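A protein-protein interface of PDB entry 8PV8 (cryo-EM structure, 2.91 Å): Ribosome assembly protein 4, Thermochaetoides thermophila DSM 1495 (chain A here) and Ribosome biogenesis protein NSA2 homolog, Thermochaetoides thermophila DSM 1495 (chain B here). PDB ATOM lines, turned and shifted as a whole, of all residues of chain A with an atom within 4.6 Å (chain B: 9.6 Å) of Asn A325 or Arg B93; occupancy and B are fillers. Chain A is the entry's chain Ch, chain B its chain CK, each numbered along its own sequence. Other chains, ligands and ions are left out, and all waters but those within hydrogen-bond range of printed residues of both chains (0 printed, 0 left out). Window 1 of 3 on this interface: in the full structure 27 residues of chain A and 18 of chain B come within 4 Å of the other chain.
The guanidinium group (NH2) of Arg B93 lies within salt-bridge range of the side-chain carboxylate (OD2) of Asp A380, at 3.2 Å. The guanidinium group of Arg B93 sits at hydrogen-bond distance from the side-chain amide oxygen of Asn A325 (3.0 Å).
The side-chain amide oxygen of Asn A325 lies close to the side-chain carboxylate of Asp A380 (3.1 Å). ND2 of Asn A325 is in hydrogen-bond range of O of Val A407, 2.9 Å away. The backbone NH of Asn A325 lies within hydrogen-bond range of the backbone carbonyl oxygen of Ala A378, at 3.2 Å. O of Tyr B89 is in hydrogen-bond range of NE of Arg B93, 2.9 Å away. N of Asp A380 is in hydrogen-bond range of O of Trp A323, 2.9 Å away. The backbone carbonyl oxygen (O) of Thr B188 lies close to the side-chain amide oxygen (OD1) of Asn B190 (3.1 Å).
Among the printed residues, merely in contact across the chains: Trp A323 with Asp B92, Trp A323 with Thr B188, Trp A323 with Leu B189, Lys A406 with Arg B93, Asn A408 with Tyr B89 and Trp A424 with Leu B90.
No residue of chain B comes within 4 Å of Val A324. Asn A325 touches just one residue of chain B: Arg B93 (3.0 Å). Printed residues of chain B within 4 Å of Asp A380: Arg B93 (3.2 Å). Printed residues of chain A within 4 Å of Tyr B89: Asn A408. Of the printed residues of chain A, Leu B90 touches Trp A424 (3.6 Å). Arg B93 touches just these residues of chain A: Asn A325 (3.0 Å), Asp A380 (3.2 Å) and Lys A406 (3.5 Å). The nearest printed residue of chain A that does not touch Tyr B89 is Trp A424 (5.0 Å).
Hydrophobic or aromatic side chains of chain B that line the printed part of chain A: Tyr B89, Leu B90 and Leu B189. Printed residues of chain A that touch a printed residue of chain B: Trp A323, Asn A325, Asp A380, Lys A406, Asn A408 and Trp A424. Among the printed residues, Asp or Glu carboxylates within 4 Å of a Lys or Arg side-chain nitrogen of the other chain: Asp A380 with Arg B93.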
ATOM      1  N   SER A 284     -25.158   4.994  14.167  1.00  0.00           N
ATOM      2  CA  SER A 284     -24.584   5.427  12.902  1.00  0.00           C
ATOM      3  C   SER A 284     -25.561   5.375  11.735  1.00  0.00           C
ATOM      4  O   SER A 284     -25.281   5.978  10.693  1.00  0.00           O
ATOM      5  CB  SER A 284     -23.354   4.577  12.566  1.00  0.00           C
ATOM      6  OG  SER A 284     -23.681   3.199  12.535  1.00  0.00           O
ATOM      7  N   CYS A 285     -26.692   4.686  11.874  1.00  0.00           N
ATOM      8  CA  CYS A 285     -27.623   4.534  10.766  1.00  0.00           C
ATOM      9  C   CYS A 285     -29.013   4.203  11.288  1.00  0.00           C
ATOM     10  O   CYS A 285     -29.166   3.397  12.213  1.00  0.00           O
ATOM     11  CB  CYS A 285     -27.145   3.451   9.791  1.00  0.00           C
ATOM     12  SG  CYS A 285     -26.875   1.832  10.541  1.00  0.00           S
ATOM     13  N   TRP A 323     -18.355  -2.415  15.009  1.00  0.00           N
ATOM     14  CA  TRP A 323     -19.263  -1.322  14.681  1.00  0.00           C
ATOM     15  C   TRP A 323     -20.145  -1.682  13.494  1.00  0.00           C
ATOM     16  O   TRP A 323     -19.679  -2.230  12.494  1.00  0.00           O
ATOM     17  CB  TRP A 323     -18.476  -0.057  14.335  1.00  0.00           C
ATOM     18  CG  TRP A 323     -17.745   0.573  15.468  1.00  0.00           C
ATOM     19  CD1 TRP A 323     -17.742   0.176  16.770  1.00  0.00           C
ATOM     20  CD2 TRP A 323     -16.895   1.720  15.394  1.00  0.00           C
ATOM     21  NE1 TRP A 323     -16.944   1.008  17.516  1.00  0.00           N
ATOM     22  CE2 TRP A 323     -16.411   1.964  16.692  1.00  0.00           C
ATOM     23  CE3 TRP A 323     -16.497   2.567  14.354  1.00  0.00           C
ATOM     24  CZ2 TRP A 323     -15.551   3.019  16.980  1.00  0.00           C
ATOM     25  CZ3 TRP A 323     -15.644   3.612  14.642  1.00  0.00           C
ATOM     26  CH2 TRP A 323     -15.180   3.830  15.944  1.00  0.00           C
ATOM     27  N   VAL A 324     -21.428  -1.356  13.604  1.00  0.00           N
ATOM     28  CA  VAL A 324     -22.359  -1.498  12.492  1.00  0.00           C
ATOM     29  C   VAL A 324     -22.384  -0.184  11.725  1.00  0.00           C
ATOM     30  O   VAL A 324     -22.949   0.812  12.194  1.00  0.00           O
ATOM     31  CB  VAL A 324     -23.762  -1.880  12.991  1.00  0.00           C
ATOM     32  CG1 VAL A 324     -24.747  -1.920  11.834  1.00  0.00           C
ATOM     33  CG2 VAL A 324     -23.721  -3.215  13.706  1.00  0.00           C
ATOM     34  N   ASN A 325     -21.753  -0.174  10.553  1.00  0.00           N
ATOM     35  CA  ASN A 325     -21.636   1.030   9.739  1.00  0.00           C
ATOM     36  C   ASN A 325     -22.926   1.405   9.029  1.00  0.00           C
ATOM     37  O   ASN A 325     -23.276   2.587   8.979  1.00  0.00           O
ATOM     38  CB  ASN A 325     -20.528   0.862   8.696  1.00  0.00           C
ATOM     39  CG  ASN A 325     -19.211   0.450   9.308  1.00  0.00           C
ATOM     40  OD1 ASN A 325     -18.879   0.852  10.421  1.00  0.00           O
ATOM     41  ND2 ASN A 325     -18.449  -0.354   8.579  1.00  0.00           N
ATOM     42  N   HIS A 326     -23.643   0.431   8.479  1.00  0.00           N
ATOM     43  CA  HIS A 326     -24.780   0.737   7.627  1.00  0.00           C
ATOM     44  C   HIS A 326     -25.763  -0.422   7.647  1.00  0.00           C
ATOM     45  O   HIS A 326     -25.385  -1.582   7.847  1.00  0.00           O
ATOM     46  CB  HIS A 326     -24.325   1.030   6.192  1.00  0.00           C
ATOM     47  CG  HIS A 326     -25.371   1.680   5.343  1.00  0.00           C
ATOM     48  ND1 HIS A 326     -26.050   1.006   4.352  1.00  0.00           N
ATOM     49  CD2 HIS A 326     -25.851   2.946   5.334  1.00  0.00           C
ATOM     50  CE1 HIS A 326     -26.904   1.828   3.769  1.00  0.00           C
ATOM     51  NE2 HIS A 326     -26.804   3.011   4.347  1.00  0.00           N
ATOM     52  N   ALA A 378     -24.321  -4.308   7.656  1.00  0.00           N
ATOM     53  CA  ALA A 378     -22.901  -4.455   7.382  1.00  0.00           C
ATOM     54  C   ALA A 378     -22.104  -3.987   8.589  1.00  0.00           C
ATOM     55  O   ALA A 378     -22.471  -2.998   9.230  1.00  0.00           O
ATOM     56  CB  ALA A 378     -22.505  -3.644   6.151  1.00  0.00           C
ATOM     57  N   SER A 379     -21.013  -4.684   8.907  1.00  0.00           N
ATOM     58  CA  SER A 379     -20.244  -4.292  10.076  1.00  0.00           C
ATOM     59  C   SER A 379     -18.754  -4.284   9.770  1.00  0.00           C
ATOM     60  O   SER A 379     -18.306  -4.735   8.715  1.00  0.00           O
ATOM     61  CB  SER A 379     -20.528  -5.204  11.271  1.00  0.00           C
ATOM     62  OG  SER A 379     -20.541  -6.564  10.877  1.00  0.00           O
ATOM     63  N   ASP A 380     -17.991  -3.752  10.727  1.00  0.00           N
ATOM     64  CA  ASP A 380     -16.536  -3.648  10.707  1.00  0.00           C
ATOM     65  C   ASP A 380     -15.851  -4.932  11.090  1.00  0.00           C
ATOM     66  O   ASP A 380     -14.615  -4.978  11.068  1.00  0.00           O
ATOM     67  CB  ASP A 380     -16.077  -2.525  11.637  1.00  0.00           C
ATOM     68  CG  ASP A 380     -16.165  -1.161  10.992  1.00  0.00           C
ATOM     69  OD1 ASP A 380     -16.554  -1.089   9.809  1.00  0.00           O
ATOM     70  OD2 ASP A 380     -15.843  -0.161  11.665  1.00  0.00           O
ATOM     71  N   LYS A 406     -13.278  -4.047   6.350  1.00  0.00           N
ATOM     72  CA  LYS A 406     -14.549  -3.515   6.821  1.00  0.00           C
ATOM     73  C   LYS A 406     -15.481  -3.243   5.648  1.00  0.00           C
ATOM     74  O   LYS A 406     -15.050  -2.803   4.579  1.00  0.00           O
ATOM     75  CB  LYS A 406     -14.317  -2.232   7.617  1.00  0.00           C
ATOM     76  CG  LYS A 406     -13.286  -2.370   8.718  1.00  0.00           C
ATOM     77  CD  LYS A 406     -13.011  -1.036   9.385  1.00  0.00           C
ATOM     78  CE  LYS A 406     -12.313  -0.084   8.436  1.00  0.00           C
ATOM     79  NZ  LYS A 406     -10.963  -0.583   8.064  1.00  0.00           N
ATOM     80  N   VAL A 407     -16.764  -3.525   5.845  1.00  0.00           N
ATOM     81  CA  VAL A 407     -17.767  -3.327   4.809  1.00  0.00           C
ATOM     82  C   VAL A 407     -18.434  -1.986   5.076  1.00  0.00           C
ATOM     83  O   VAL A 407     -19.039  -1.785   6.137  1.00  0.00           O
ATOM     84  CB  VAL A 407     -18.795  -4.467   4.789  1.00  0.00           C
ATOM     85  CG1 VAL A 407     -19.864  -4.187   3.748  1.00  0.00           C
ATOM     86  CG2 VAL A 407     -18.112  -5.792   4.538  1.00  0.00           C
ATOM     87  N   ASN A 408     -18.327  -1.068   4.119  1.00  0.00           N
ATOM     88  CA  ASN A 408     -18.759   0.306   4.345  1.00  0.00           C
ATOM     89  C   ASN A 408     -20.220   0.534   3.983  1.00  0.00           C
ATOM     90  O   ASN A 408     -20.980   1.070   4.797  1.00  0.00           O
ATOM     91  CB  ASN A 408     -17.873   1.267   3.549  1.00  0.00           C
ATOM     92  CG  ASN A 408     -17.914   2.676   4.093  1.00  0.00           C
ATOM     93  OD1 ASN A 408     -17.485   2.934   5.217  1.00  0.00           O
ATOM     94  ND2 ASN A 408     -18.431   3.603   3.295  1.00  0.00           N
ATOM     95  N   TRP A 424     -13.875  -2.065   2.337  1.00  0.00           N
ATOM     96  CA  TRP A 424     -12.571  -1.427   2.450  1.00  0.00           C
ATOM     97  C   TRP A 424     -11.454  -2.284   1.874  1.00  0.00           C
ATOM     98  O   TRP A 424     -10.290  -1.872   1.914  1.00  0.00           O
ATOM     99  CB  TRP A 424     -12.263  -1.088   3.911  1.00  0.00           C
ATOM    100  CG  TRP A 424     -13.040   0.074   4.462  1.00  0.00           C
ATOM    101  CD1 TRP A 424     -14.396   0.218   4.493  1.00  0.00           C
ATOM    102  CD2 TRP A 424     -12.500   1.254   5.071  1.00  0.00           C
ATOM    103  NE1 TRP A 424     -14.733   1.413   5.079  1.00  0.00           N
ATOM    104  CE2 TRP A 424     -13.587   2.067   5.442  1.00  0.00           C
ATOM    105  CE3 TRP A 424     -11.202   1.700   5.336  1.00  0.00           C
ATOM    106  CZ2 TRP A 424     -13.417   3.301   6.065  1.00  0.00           C
ATOM    107  CZ3 TRP A 424     -11.035   2.925   5.953  1.00  0.00           C
ATOM    108  CH2 TRP A 424     -12.136   3.711   6.311  1.00  0.00           C
ATOM    109  N   PRO B  82     -13.234  17.512  14.086  1.00  0.00           N
ATOM    110  CA  PRO B  82     -12.015  17.421  13.272  1.00  0.00           C
ATOM    111  C   PRO B  82     -11.782  18.669  12.431  1.00  0.00           C
ATOM    112  O   PRO B  82     -12.672  19.495  12.222  1.00  0.00           O
ATOM    113  CB  PRO B  82     -12.269  16.202  12.371  1.00  0.00           C
ATOM    114  CG  PRO B  82     -13.550  15.579  12.839  1.00  0.00           C
ATOM    115  CD  PRO B  82     -13.992  16.251  14.090  1.00  0.00           C
ATOM    116  N   ILE B  86     -15.268  15.274   6.900  1.00  0.00           N
ATOM    117  CA  ILE B  86     -15.369  13.873   6.499  1.00  0.00           C
ATOM    118  C   ILE B  86     -16.823  13.456   6.667  1.00  0.00           C
ATOM    119  O   ILE B  86     -17.551  14.026   7.496  1.00  0.00           O
ATOM    120  CB  ILE B  86     -14.409  12.974   7.314  1.00  0.00           C
ATOM    121  CG1 ILE B  86     -14.576  13.232   8.811  1.00  0.00           C
ATOM    122  CG2 ILE B  86     -12.966  13.180   6.872  1.00  0.00           C
ATOM    123  CD1 ILE B  86     -13.713  12.349   9.682  1.00  0.00           C
ATOM    124  N   PRO B  87     -17.289  12.477   5.889  1.00  0.00           N
ATOM    125  CA  PRO B  87     -18.682  12.027   6.024  1.00  0.00           C
ATOM    126  C   PRO B  87     -18.922  11.290   7.334  1.00  0.00           C
ATOM    127  O   PRO B  87     -18.019  11.066   8.142  1.00  0.00           O
ATOM    128  CB  PRO B  87     -18.889  11.101   4.821  1.00  0.00           C
ATOM    129  CG  PRO B  87     -17.780  11.404   3.888  1.00  0.00           C
ATOM    130  CD  PRO B  87     -16.633  11.878   4.713  1.00  0.00           C
ATOM    131  N   SER B  88     -20.188  10.910   7.532  1.00  0.00           N
ATOM    132  CA  SER B  88     -20.599  10.311   8.799  1.00  0.00           C
ATOM    133  C   SER B  88     -20.019   8.916   8.989  1.00  0.00           C
ATOM    134  O   SER B  88     -19.824   8.478  10.128  1.00  0.00           O
ATOM    135  CB  SER B  88     -22.124  10.263   8.884  1.00  0.00           C
ATOM    136  OG  SER B  88     -22.666   9.457   7.854  1.00  0.00           O
ATOM    137  N   TYR B  89     -19.739   8.202   7.900  1.00  0.00           N
ATOM    138  CA  TYR B  89     -19.171   6.865   8.017  1.00  0.00           C
ATOM    139  C   TYR B  89     -17.664   6.879   8.233  1.00  0.00           C
ATOM    140  O   TYR B  89     -17.078   5.814   8.454  1.00  0.00           O
ATOM    141  CB  TYR B  89     -19.520   6.025   6.782  1.00  0.00           C
ATOM    142  CG  TYR B  89     -19.253   6.685   5.444  1.00  0.00           C
ATOM    143  CD1 TYR B  89     -17.971   6.734   4.908  1.00  0.00           C
ATOM    144  CD2 TYR B  89     -20.291   7.239   4.707  1.00  0.00           C
ATOM    145  CE1 TYR B  89     -17.730   7.329   3.684  1.00  0.00           C
ATOM    146  CE2 TYR B  89     -20.059   7.834   3.483  1.00  0.00           C
ATOM    147  CZ  TYR B  89     -18.778   7.876   2.977  1.00  0.00           C
ATOM    148  OH  TYR B  89     -18.544   8.468   1.759  1.00  0.00           O
ATOM    149  N   LEU B  90     -17.024   8.046   8.177  1.00  0.00           N
ATOM    150  CA  LEU B  90     -15.603   8.174   8.462  1.00  0.00           C
ATOM    151  C   LEU B  90     -15.336   8.844   9.802  1.00  0.00           C
ATOM    152  O   LEU B  90     -14.173   9.057  10.158  1.00  0.00           O
ATOM    153  CB  LEU B  90     -14.904   8.944   7.341  1.00  0.00           C
ATOM    154  CG  LEU B  90     -14.779   8.195   6.015  1.00  0.00           C
ATOM    155  CD1 LEU B  90     -14.097   9.059   4.969  1.00  0.00           C
ATOM    156  CD2 LEU B  90     -14.023   6.895   6.213  1.00  0.00           C
ATOM    157  N   LEU B  91     -16.384   9.180  10.551  1.00  0.00           N
ATOM    158  CA  LEU B  91     -16.216   9.778  11.864  1.00  0.00           C
ATOM    159  C   LEU B  91     -15.765   8.732  12.878  1.00  0.00           C
ATOM    160  O   LEU B  91     -15.955   7.526  12.693  1.00  0.00           O
ATOM    161  CB  LEU B  91     -17.517  10.431  12.330  1.00  0.00           C
ATOM    162  CG  LEU B  91     -17.991  11.639  11.524  1.00  0.00           C
ATOM    163  CD1 LEU B  91     -19.355  12.096  12.006  1.00  0.00           C
ATOM    164  CD2 LEU B  91     -16.981  12.769  11.626  1.00  0.00           C
ATOM    165  N   ASP B  92     -15.139   9.219  13.952  1.00  0.00           N
ATOM    166  CA  ASP B  92     -14.611   8.440  15.073  1.00  0.00           C
ATOM    167  C   ASP B  92     -13.571   7.410  14.650  1.00  0.00           C
ATOM    168  O   ASP B  92     -13.375   6.416  15.358  1.00  0.00           O
ATOM    169  CB  ASP B  92     -15.726   7.741  15.861  1.00  0.00           C
ATOM    170  CG  ASP B  92     -16.655   8.721  16.549  1.00  0.00           C
ATOM    171  OD1 ASP B  92     -17.432   8.289  17.425  1.00  0.00           O
ATOM    172  OD2 ASP B  92     -16.606   9.923  16.213  1.00  0.00           O
ATOM    173  N   ARG B  93     -12.893   7.620  13.527  1.00  0.00           N
ATOM    174  CA  ARG B  93     -11.874   6.708  13.035  1.00  0.00           C
ATOM    175  C   ARG B  93     -10.511   7.386  13.057  1.00  0.00           C
ATOM    176  O   ARG B  93     -10.398   8.614  12.987  1.00  0.00           O
ATOM    177  CB  ARG B  93     -12.199   6.231  11.616  1.00  0.00           C
ATOM    178  CG  ARG B  93     -13.525   5.506  11.493  1.00  0.00           C
ATOM    179  CD  ARG B  93     -13.774   5.051  10.067  1.00  0.00           C
ATOM    180  NE  ARG B  93     -15.040   4.341   9.934  1.00  0.00           N
ATOM    181  CZ  ARG B  93     -15.179   3.029  10.062  1.00  0.00           C
ATOM    182  NH1 ARG B  93     -14.146   2.246  10.325  1.00  0.00           N
ATOM    183  NH2 ARG B  93     -16.386   2.489   9.920  1.00  0.00           N
ATOM    184  N   ALA B  94      -9.470   6.566  13.159  1.00  0.00           N
ATOM    185  CA  ALA B  94      -8.103   7.067  13.189  1.00  0.00           C
ATOM    186  C   ALA B  94      -7.667   7.541  11.806  1.00  0.00           C
ATOM    187  O   ALA B  94      -6.986   8.557  11.674  1.00  0.00           O
ATOM    188  CB  ALA B  94      -7.157   5.996  13.705  1.00  0.00           C
ATOM    189  N   PRO B 187      -8.797  -1.387  21.511  1.00  0.00           N
ATOM    190  CA  PRO B 187      -8.558   0.042  21.223  1.00  0.00           C
ATOM    191  C   PRO B 187      -9.627   0.697  20.363  1.00  0.00           C
ATOM    192  O   PRO B 187      -9.906   1.891  20.531  1.00  0.00           O
ATOM    193  CB  PRO B 187      -7.194   0.023  20.520  1.00  0.00           C
ATOM    194  CG  PRO B 187      -6.549  -1.239  20.965  1.00  0.00           C
ATOM    195  CD  PRO B 187      -7.660  -2.230  21.113  1.00  0.00           C
ATOM    196  N   THR B 188     -10.236  -0.049  19.441  1.00  0.00           N
ATOM    197  CA  THR B 188     -11.216   0.556  18.546  1.00  0.00           C
ATOM    198  C   THR B 188     -12.624   0.487  19.125  1.00  0.00           C
ATOM    199  O   THR B 188     -13.357   1.482  19.100  1.00  0.00           O
ATOM    200  CB  THR B 188     -11.168  -0.120  17.178  1.00  0.00           C
ATOM    201  OG1 THR B 188      -9.811  -0.183  16.726  1.00  0.00           O
ATOM    202  CG2 THR B 188     -11.982   0.674  16.172  1.00  0.00           C
ATOM    203  N   LEU B 189     -13.018  -0.674  19.653  1.00  0.00           N
ATOM    204  CA  LEU B 189     -14.350  -0.830  20.226  1.00  0.00           C
ATOM    205  C   LEU B 189     -14.510  -0.110  21.557  1.00  0.00           C
ATOM    206  O   LEU B 189     -15.652   0.142  21.961  1.00  0.00           O
ATOM    207  CB  LEU B 189     -14.671  -2.314  20.407  1.00  0.00           C
ATOM    208  CG  LEU B 189     -15.276  -3.037  19.207  1.00  0.00           C
ATOM    209  CD1 LEU B 189     -15.352  -4.527  19.478  1.00  0.00           C
ATOM    210  CD2 LEU B 189     -16.649  -2.478  18.891  1.00  0.00           C
ATOM    211  N   ASN B 190     -13.402   0.215  22.229  1.00  0.00           N
ATOM    212  CA  ASN B 190     -13.383   0.918  23.516  1.00  0.00           C
ATOM    213  C   ASN B 190     -14.182   0.167  24.581  1.00  0.00           C
ATOM    214  O   ASN B 190     -14.900   0.755  25.391  1.00  0.00           O
ATOM    215  CB  ASN B 190     -13.875   2.358  23.367  1.00  0.00           C
ATOM    216  CG  ASN B 190     -12.976   3.186  22.474  1.00  0.00           C
ATOM    217  OD1 ASN B 190     -13.383   3.625  21.399  1.00  0.00           O
ATOM    218  ND2 ASN B 190     -11.737   3.382  22.903  1.00  0.00           N
